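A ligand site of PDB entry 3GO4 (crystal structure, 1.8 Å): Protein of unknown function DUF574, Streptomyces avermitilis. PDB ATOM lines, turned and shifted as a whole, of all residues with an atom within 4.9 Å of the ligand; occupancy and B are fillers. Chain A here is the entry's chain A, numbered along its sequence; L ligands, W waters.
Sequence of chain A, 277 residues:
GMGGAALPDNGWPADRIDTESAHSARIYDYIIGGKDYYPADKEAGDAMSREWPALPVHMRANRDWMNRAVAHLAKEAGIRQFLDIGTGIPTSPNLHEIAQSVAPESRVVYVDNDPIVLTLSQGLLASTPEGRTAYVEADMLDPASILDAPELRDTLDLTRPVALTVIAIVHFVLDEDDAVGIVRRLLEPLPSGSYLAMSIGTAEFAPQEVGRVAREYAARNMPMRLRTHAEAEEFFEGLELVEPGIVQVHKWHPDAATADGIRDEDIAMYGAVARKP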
ATOM      1  N   SER A  24     -21.067  17.503   9.452  1.00  0.00           N
ATOM      2  CA  SER A  24     -21.683  17.094  10.722  1.00  0.00           C
ATOM      3  C   SER A  24     -21.302  15.713  11.230  1.00  0.00           C
ATOM      4  O   SER A  24     -21.087  15.554  12.439  1.00  0.00           O
ATOM      5  CB  SER A  24     -23.208  17.205  10.636  1.00  0.00           C
ATOM      6  OG  SER A  24     -23.764  16.283   9.712  1.00  0.00           O
ATOM      7  N   ALA A  25     -21.210  14.733  10.333  1.00  0.00           N
ATOM      8  CA  ALA A  25     -20.840  13.370  10.726  1.00  0.00           C
ATOM      9  C   ALA A  25     -19.445  13.268  11.340  1.00  0.00           C
ATOM     10  O   ALA A  25     -19.207  12.490  12.249  1.00  0.00           O
ATOM     11  CB  ALA A  25     -20.944  12.391   9.525  1.00  0.00           C
ATOM     12  N   TYR A  28     -19.117  15.250  14.701  1.00  0.00           N
ATOM     13  CA  TYR A  28     -19.695  14.234  15.644  1.00  0.00           C
ATOM     14  C   TYR A  28     -18.688  13.147  15.989  1.00  0.00           C
ATOM     15  O   TYR A  28     -18.449  12.861  17.151  1.00  0.00           O
ATOM     16  CB  TYR A  28     -20.987  13.639  15.028  1.00  0.00           C
ATOM     17  CG  TYR A  28     -21.757  12.596  15.834  1.00  0.00           C
ATOM     18  CD1 TYR A  28     -22.081  12.803  17.161  1.00  0.00           C
ATOM     19  CD2 TYR A  28     -22.263  11.435  15.225  1.00  0.00           C
ATOM     20  CE1 TYR A  28     -22.827  11.871  17.889  1.00  0.00           C
ATOM     21  CE2 TYR A  28     -23.003  10.486  15.967  1.00  0.00           C
ATOM     22  CZ  TYR A  28     -23.294  10.732  17.292  1.00  0.00           C
ATOM     23  OH  TYR A  28     -24.053   9.851  18.042  1.00  0.00           O
ATOM     24  N   ASN A  62     -26.257  10.959  23.187  1.00  0.00           N
ATOM     25  CA  ASN A  62     -27.050  10.669  22.001  1.00  0.00           C
ATOM     26  C   ASN A  62     -26.683   9.284  21.439  1.00  0.00           C
ATOM     27  O   ASN A  62     -27.532   8.401  21.265  1.00  0.00           O
ATOM     28  CB  ASN A  62     -26.810  11.734  20.904  1.00  0.00           C
ATOM     29  CG  ASN A  62     -27.602  11.434  19.624  1.00  0.00           C
ATOM     30  OD1 ASN A  62     -28.826  11.668  19.531  1.00  0.00           O
ATOM     31  ND2 ASN A  62     -26.919  10.867  18.631  1.00  0.00           N
ATOM     32  N   ARG A  63     -25.394   9.059  21.227  1.00  0.00           N
ATOM     33  CA  ARG A  63     -24.946   7.778  20.721  1.00  0.00           C
ATOM     34  C   ARG A  63     -25.343   6.644  21.682  1.00  0.00           C
ATOM     35  O   ARG A  63     -25.740   5.605  21.223  1.00  0.00           O
ATOM     36  CB  ARG A  63     -23.449   7.750  20.459  1.00  0.00           C
ATOM     37  CG  ARG A  63     -22.941   6.468  19.715  1.00  0.00           C
ATOM     38  CD  ARG A  63     -23.496   6.372  18.334  1.00  0.00           C
ATOM     39  NE  ARG A  63     -23.004   5.187  17.580  1.00  0.00           N
ATOM     40  CZ  ARG A  63     -23.152   5.042  16.279  1.00  0.00           C
ATOM     41  NH1 ARG A  63     -23.740   5.984  15.561  1.00  0.00           N
ATOM     42  NH2 ARG A  63     -22.678   3.970  15.653  1.00  0.00           N
ATOM     43  N   ASP A  84     -32.462   3.188   8.827  1.00  0.00           N
ATOM     44  CA  ASP A  84     -31.730   4.224   9.597  1.00  0.00           C
ATOM     45  C   ASP A  84     -31.337   5.372   8.694  1.00  0.00           C
ATOM     46  O   ASP A  84     -30.549   5.169   7.786  1.00  0.00           O
ATOM     47  CB  ASP A  84     -30.503   3.589  10.178  1.00  0.00           C
ATOM     48  CG  ASP A  84     -29.729   4.474  11.137  1.00  0.00           C
ATOM     49  OD1 ASP A  84     -30.289   5.112  12.069  1.00  0.00           O
ATOM     50  OD2 ASP A  84     -28.499   4.420  11.022  1.00  0.00           O
ATOM     51  N   ILE A  85     -31.901   6.543   8.971  1.00  0.00           N
ATOM     52  CA  ILE A  85     -31.691   7.731   8.157  1.00  0.00           C
ATOM     53  C   ILE A  85     -30.741   8.669   8.892  1.00  0.00           C
ATOM     54  O   ILE A  85     -31.031   9.129  10.009  1.00  0.00           O
ATOM     55  CB  ILE A  85     -33.025   8.431   7.798  1.00  0.00           C
ATOM     56  CG1 ILE A  85     -34.076   7.438   7.313  1.00  0.00           C
ATOM     57  CG2 ILE A  85     -32.841   9.559   6.710  1.00  0.00           C
ATOM     58  CD1 ILE A  85     -33.692   6.574   6.128  1.00  0.00           C
ATOM     59  N   GLY A  86     -29.633   8.988   8.231  1.00  0.00           N
ATOM     60  CA  GLY A  86     -28.565   9.806   8.781  1.00  0.00           C
ATOM     61  C   GLY A  86     -27.723   8.892   9.652  1.00  0.00           C
ATOM     62  O   GLY A  86     -27.506   9.175  10.842  1.00  0.00           O
ATOM     63  N   THR A  87     -27.251   7.814   9.034  1.00  0.00           N
ATOM     64  CA  THR A  87     -26.493   6.810   9.733  1.00  0.00           C
ATOM     65  C   THR A  87     -25.219   7.328  10.365  1.00  0.00           C
ATOM     66  O   THR A  87     -24.860   6.890  11.444  1.00  0.00           O
ATOM     67  CB  THR A  87     -26.148   5.607   8.809  1.00  0.00           C
ATOM     68  OG1 THR A  87     -27.380   4.981   8.422  1.00  0.00           O
ATOM     69  CG2 THR A  87     -25.271   4.549   9.559  1.00  0.00           C
ATOM     70  N   GLY A  88     -24.539   8.274   9.745  1.00  0.00           N
ATOM     71  CA  GLY A  88     -23.255   8.687  10.315  1.00  0.00           C
ATOM     72  C   GLY A  88     -22.130   7.693  10.128  1.00  0.00           C
ATOM     73  O   GLY A  88     -22.286   6.574   9.578  1.00  0.00           O
ATOM     74  N   ILE A  89     -20.954   8.146  10.554  1.00  0.00           N
ATOM     75  CA  ILE A  89     -19.746   7.380  10.436  1.00  0.00           C
ATOM     76  C   ILE A  89     -19.871   6.183  11.363  1.00  0.00           C
ATOM     77  O   ILE A  89     -20.323   6.321  12.462  1.00  0.00           O
ATOM     78  CB  ILE A  89     -18.542   8.252  10.793  1.00  0.00           C
ATOM     79  CG1 ILE A  89     -18.312   9.274   9.651  1.00  0.00           C
ATOM     80  CG2 ILE A  89     -17.297   7.433  11.034  1.00  0.00           C
ATOM     81  CD1 ILE A  89     -17.323  10.366  10.006  1.00  0.00           C
ATOM     82  N   VAL A 111     -28.519   4.593   5.787  1.00  0.00           N
ATOM     83  CA  VAL A 111     -28.613   5.658   4.779  1.00  0.00           C
ATOM     84  C   VAL A 111     -27.928   6.967   5.209  1.00  0.00           C
ATOM     85  O   VAL A 111     -28.131   7.431   6.335  1.00  0.00           O
ATOM     86  CB  VAL A 111     -30.120   5.970   4.554  1.00  0.00           C
ATOM     87  CG1 VAL A 111     -30.297   6.951   3.416  1.00  0.00           C
ATOM     88  CG2 VAL A 111     -30.982   4.648   4.337  1.00  0.00           C
ATOM     89  N   ASP A 112     -27.131   7.592   4.321  1.00  0.00           N
ATOM     90  CA  ASP A 112     -26.501   8.846   4.687  1.00  0.00           C
ATOM     91  C   ASP A 112     -26.210   9.573   3.397  1.00  0.00           C
ATOM     92  O   ASP A 112     -26.162   8.936   2.337  1.00  0.00           O
ATOM     93  CB  ASP A 112     -25.221   8.634   5.521  1.00  0.00           C
ATOM     94  CG  ASP A 112     -24.942   9.788   6.500  1.00  0.00           C
ATOM     95  OD1 ASP A 112     -24.501  10.847   6.070  1.00  0.00           O
ATOM     96  OD2 ASP A 112     -25.134   9.641   7.740  1.00  0.00           O
ATOM     97  N   ASN A 113     -26.098  10.896   3.459  1.00  0.00           N
ATOM     98  CA  ASN A 113     -25.701  11.668   2.288  1.00  0.00           C
ATOM     99  C   ASN A 113     -24.270  12.226   2.382  1.00  0.00           C
ATOM    100  O   ASN A 113     -23.869  13.004   1.529  1.00  0.00           O
ATOM    101  CB  ASN A 113     -26.674  12.801   1.983  1.00  0.00           C
ATOM    102  CG  ASN A 113     -26.606  13.944   2.994  1.00  0.00           C
ATOM    103  OD1 ASN A 113     -25.972  13.839   4.036  1.00  0.00           O
ATOM    104  ND2 ASN A 113     -27.264  15.043   2.673  1.00  0.00           N
ATOM    105  N   ASP A 114     -23.506  11.867   3.397  1.00  0.00           N
ATOM    106  CA  ASP A 114     -22.118  12.338   3.469  1.00  0.00           C
ATOM    107  C   ASP A 114     -21.237  11.325   2.714  1.00  0.00           C
ATOM    108  O   ASP A 114     -21.167  10.208   3.129  1.00  0.00           O
ATOM    109  CB  ASP A 114     -21.663  12.500   4.926  1.00  0.00           C
ATOM    110  CG  ASP A 114     -20.268  13.113   5.039  1.00  0.00           C
ATOM    111  OD1 ASP A 114     -19.453  12.906   4.097  1.00  0.00           O
ATOM    112  OD2 ASP A 114     -19.979  13.794   6.081  1.00  0.00           O
ATOM    113  N   VAL A 117     -19.278   8.495   4.435  1.00  0.00           N
ATOM    114  CA  VAL A 117     -19.896   7.281   5.014  1.00  0.00           C
ATOM    115  C   VAL A 117     -19.708   6.077   4.067  1.00  0.00           C
ATOM    116  O   VAL A 117     -19.405   4.965   4.525  1.00  0.00           O
ATOM    117  CB  VAL A 117     -21.390   7.467   5.440  1.00  0.00           C
ATOM    118  CG1 VAL A 117     -21.899   6.140   6.075  1.00  0.00           C
ATOM    119  CG2 VAL A 117     -21.569   8.640   6.467  1.00  0.00           C
ATOM    120  N   ALA A 138     -28.021   8.609  -0.027  1.00  0.00           N
ATOM    121  CA  ALA A 138     -29.218   9.287  -0.458  1.00  0.00           C
ATOM    122  C   ALA A 138     -29.598  10.389   0.523  1.00  0.00           C
ATOM    123  O   ALA A 138     -29.168  10.380   1.677  1.00  0.00           O
ATOM    124  CB  ALA A 138     -30.369   8.284  -0.572  1.00  0.00           C
ATOM    125  N   ASP A 139     -30.421  11.312   0.039  1.00  0.00           N
ATOM    126  CA  ASP A 139     -30.873  12.484   0.792  1.00  0.00           C
ATOM    127  C   ASP A 139     -32.282  12.243   1.355  1.00  0.00           C
ATOM    128  O   ASP A 139     -33.211  11.900   0.601  1.00  0.00           O
ATOM    129  CB  ASP A 139     -30.844  13.687  -0.165  1.00  0.00           C
ATOM    130  CG  ASP A 139     -31.126  15.021   0.505  1.00  0.00           C
ATOM    131  OD1 ASP A 139     -31.695  15.053   1.614  1.00  0.00           O
ATOM    132  OD2 ASP A 139     -30.803  16.078  -0.116  1.00  0.00           O
ATOM    133  N   MET A 140     -32.457  12.404   2.682  1.00  0.00           N
ATOM    134  CA  MET A 140     -33.780  12.156   3.285  1.00  0.00           C
ATOM    135  C   MET A 140     -34.882  13.067   2.717  1.00  0.00           C
ATOM    136  O   MET A 140     -36.066  12.729   2.773  1.00  0.00           O
ATOM    137  CB  MET A 140     -33.756  12.185   4.837  1.00  0.00           C
ATOM    138  CG  MET A 140     -34.166  13.447   5.540  1.00  0.00           C
ATOM    139  SD  MET A 140     -34.178  13.173   7.517  1.00  0.00           S
ATOM    140  CE  MET A 140     -35.201  11.590   7.678  1.00  0.00           C
ATOM    141  N   LEU A 141     -34.485  14.198   2.141  1.00  0.00           N
ATOM    142  CA  LEU A 141     -35.438  15.076   1.470  1.00  0.00           C
ATOM    143  C   LEU A 141     -35.971  14.439   0.168  1.00  0.00           C
ATOM    144  O   LEU A 141     -36.793  15.018  -0.513  1.00  0.00           O
ATOM    145  CB  LEU A 141     -34.843  16.468   1.226  1.00  0.00           C
ATOM    146  CG  LEU A 141     -34.940  17.395   2.446  1.00  0.00           C
ATOM    147  CD1 LEU A 141     -34.328  16.789   3.712  1.00  0.00           C
ATOM    148  CD2 LEU A 141     -34.328  18.747   2.164  1.00  0.00           C
ATOM    149  N   ILE A 167     -32.095   9.544  13.872  1.00  0.00           N
ATOM    150  CA  ILE A 167     -31.408   9.979  15.051  1.00  0.00           C
ATOM    151  C   ILE A 167     -30.351  11.029  14.828  1.00  0.00           C
ATOM    152  O   ILE A 167     -29.418  10.825  14.077  1.00  0.00           O
ATOM    153  CB  ILE A 167     -30.782   8.739  15.765  1.00  0.00           C
ATOM    154  CG1 ILE A 167     -31.861   7.642  15.887  1.00  0.00           C
ATOM    155  CG2 ILE A 167     -30.109   9.121  17.153  1.00  0.00           C
ATOM    156  CD1 ILE A 167     -31.495   6.381  16.703  1.00  0.00           C
ATOM    157  N   ALA A 168     -30.529  12.144  15.539  1.00  0.00           N
ATOM    158  CA  ALA A 168     -29.554  13.245  15.534  1.00  0.00           C
ATOM    159  C   ALA A 168     -29.401  13.796  14.161  1.00  0.00           C
ATOM    160  O   ALA A 168     -28.275  14.121  13.771  1.00  0.00           O
ATOM    161  CB  ALA A 168     -28.204  12.799  15.953  1.00  0.00           C
ATOM    162  N   ILE A 169     -30.498  13.812  13.415  1.00  0.00           N
ATOM    163  CA  ILE A 169     -30.445  14.368  12.050  1.00  0.00           C
ATOM    164  C   ILE A 169     -31.478  15.444  11.790  1.00  0.00           C
ATOM    165  O   ILE A 169     -31.172  16.430  11.040  1.00  0.00           O
ATOM    166  CB  ILE A 169     -30.548  13.248  10.972  1.00  0.00           C
ATOM    167  CG1 ILE A 169     -30.671  13.864   9.548  1.00  0.00           C
ATOM    168  CG2 ILE A 169     -31.774  12.445  11.160  1.00  0.00           C
ATOM    169  CD1 ILE A 169     -30.556  12.867   8.445  1.00  0.00           C
ATOM    170  N   PHE A 172     -30.978  19.253  11.471  1.00  0.00           N
ATOM    171  CA  PHE A 172     -30.405  19.862  10.235  1.00  0.00           C
ATOM    172  C   PHE A 172     -31.453  20.093   9.153  1.00  0.00           C
ATOM    173  O   PHE A 172     -31.113  20.528   8.015  1.00  0.00           O
ATOM    174  CB  PHE A 172     -29.289  19.000   9.665  1.00  0.00           C
ATOM    175  CG  PHE A 172     -28.106  18.860  10.567  1.00  0.00           C
ATOM    176  CD1 PHE A 172     -27.244  19.920  10.770  1.00  0.00           C
ATOM    177  CD2 PHE A 172     -27.845  17.674  11.213  1.00  0.00           C
ATOM    178  CE1 PHE A 172     -26.122  19.800  11.598  1.00  0.00           C
ATOM    179  CE2 PHE A 172     -26.737  17.552  12.036  1.00  0.00           C
ATOM    180  CZ  PHE A 172     -25.897  18.615  12.236  1.00  0.00           C
HETATM  181  N1  LIG L   1     -27.727   8.702  13.493  1.00  0.00           N
HETATM  182  C1  LIG L   1     -26.273   8.730  13.963  1.00  0.00           C
HETATM  183  C2  LIG L   1     -25.437   9.825  13.285  1.00  0.00           C
HETATM  184  C3  LIG L   1     -25.893  11.250  13.618  1.00  0.00           C
HETATM  185  S1  LIG L   1     -24.959  12.508  12.778  1.00  0.00           S
HETATM  186  C4  LIG L   1     -26.238   8.892  15.476  1.00  0.00           C
HETATM  187  O1  LIG L   1     -25.359   8.407  16.175  1.00  0.00           O
HETATM  188  O2  LIG L   1     -27.144   9.488  16.052  1.00  0.00           O
HETATM  189  C5  LIG L   1     -26.008  13.199  11.538  1.00  0.00           C
HETATM  190  C6  LIG L   1     -25.876  12.441  10.235  1.00  0.00           C
HETATM  191  O3  LIG L   1     -26.971  12.784   9.374  1.00  0.00           O
HETATM  192  C7  LIG L   1     -24.594  12.789   9.483  1.00  0.00           C
HETATM  193  O4  LIG L   1     -23.929  11.586   9.156  1.00  0.00           O
HETATM  194  C8  LIG L   1     -25.069  13.522   8.252  1.00  0.00           C
HETATM  195  O5  LIG L   1     -24.239  13.386   7.113  1.00  0.00           O
HETATM  196  C9  LIG L   1     -26.447  12.903   8.062  1.00  0.00           C
HETATM  197  N2  LIG L   1     -27.362  13.723   7.271  1.00  0.00           N
HETATM  198  C10 LIG L   1     -27.565  15.042   7.409  1.00  0.00           C
HETATM  199  N3  LIG L   1     -28.491  15.486   6.520  1.00  0.00           N
HETATM  200  C11 LIG L   1     -28.877  14.427   5.798  1.00  0.00           C
HETATM  201  C12 LIG L   1     -29.835  14.202   4.710  1.00  0.00           C
HETATM  202  N4  LIG L   1     -30.543  15.256   4.257  1.00  0.00           N
HETATM  203  N5  LIG L   1     -29.955  12.944   4.218  1.00  0.00           N
HETATM  204  C13 LIG L   1     -29.254  11.898   4.736  1.00  0.00           C
HETATM  205  N6  LIG L   1     -28.351  12.037   5.726  1.00  0.00           N
HETATM  206  C14 LIG L   1     -28.148  13.249   6.304  1.00  0.00           C
HETATM  207  O   HOH W   1     -30.562   7.907  12.264  1.00  0.00           O
HETATM  208  O   HOH W   2     -28.550   6.035  14.097  1.00  0.00           O
HETATM  209  O   HOH W   3     -24.780  15.894   5.165  1.00  0.00           O
HETATM  210  O   HOH W   4     -25.503  17.411   7.806  1.00  0.00           O
HETATM  211  O   HOH W   5     -22.032  15.045   7.384  1.00  0.00           O
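OD2 of Asp 112 lies within hydrogen-bond range of O4 of the ligand.
N of Gly 88 lies close to O4 of the ligand (3.4 Å).
N6 of the ligand lies close to OD1 of Asn 113 (3.4 Å).
A nitrogen (N1) of the ligand sits at hydrogen-bond distance from the backbone carbonyl oxygen (O) of Gly 86.
The guanidinium group (NH1) of Arg 63 is in salt-bridge range of an oxygen (O1) of the ligand (3.0 Å).
N6 of the ligand lies within hydrogen-bond range of N of Asn 113, 3.4 Å away.
The backbone NH (N) of Met 140 lies within hydrogen-bond range of a nitrogen (N5) of the ligand, 3.0 Å away.
O of Ile 167 sits at hydrogen-bond distance from N1 of the ligand (2.8 Å).
OD1 of Asp 139 is in hydrogen-bond range of N4 of the ligand (2.9 Å).
An oxygen (O1) of the ligand is in hydrogen-bond range of the side-chain hydroxyl (OH) of Tyr 28, 2.7 Å away.
An oxygen (O2) of the ligand sits at hydrogen-bond distance from the side-chain amide nitrogen (ND2) of Asn 62, at 2.9 Å.
The side-chain hydroxyl of Thr 87 is in hydrogen-bond range of the side-chain carboxylate of Asp 84, 2.9 Å away.
The side-chain hydroxyl of Tyr 28 sits at hydrogen-bond distance from the side-chain amide nitrogen of Asn 62 (3.1 Å).
The backbone NH (N) of Thr 87 is in hydrogen-bond range of the side-chain carboxylate (OD2) of Asp 112, 3.1 Å away.
The backbone NH (N) of Thr 87 lies within hydrogen-bond range of the backbone carbonyl oxygen (O) of Val 111 (2.9 Å).
The backbone carbonyl oxygen (O) of Asp 112 lies within hydrogen-bond range of the backbone NH (N) of Ala 138, 3.0 Å away.
OD1 of Asp 139 lies within hydrogen-bond range of N of Leu 141 (3.0 Å).
The side-chain carboxylate (OD1) of Asp 112 is in hydrogen-bond range of the backbone NH (N) of Asp 114 (3.0 Å).
OD2 of Asp 112 lies within hydrogen-bond range of N of Gly 88 (2.5 Å).
Ser 24 touches the ligand (OG to C8, 3.4 Å).
CB of Ala 25 touches O4 of the ligand, 3.1 Å away.
O of Thr 87 touches C1 of the ligand (3.4 Å).
Asp 114 touches the ligand.
Ala 138 touches the ligand.
Ala 168 touches the ligand (O to C5, 3.3 Å).
Ile 169 touches the ligand (CD1 to C14, 3.2 Å).
Hydrophobic or aromatic side chains that line the ligand: Ala 25, Tyr 28, Met 140, Ile 167, Ala 168 and Ile 169.
Of the 24 residues printed, 17 come within 4 Å of the ligand.
The nearest printed residue that does not touch the ligand is Leu 141 (4.1 Å).
Water W5 lies within hydrogen-bond range of the side-chain carboxylate of Asp 114, an oxygen (O5) of the ligand, the backbone NH of Ala 25 and the side-chain hydroxyl of Ser 24.
Water W2 bridges OD1 of Asp 84 and N1 of the ligand.
Water W1 lies within hydrogen-bond range of O of Ile 85 (2.6 Å), N of Ile 167 (2.8 Å), OD1 of Asp 84 (2.8 Å) and N1 of the ligand (3.2 Å).
Water W3 bridges the side-chain amide oxygen of Asn 113 and an oxygen (O5) of the ligand.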
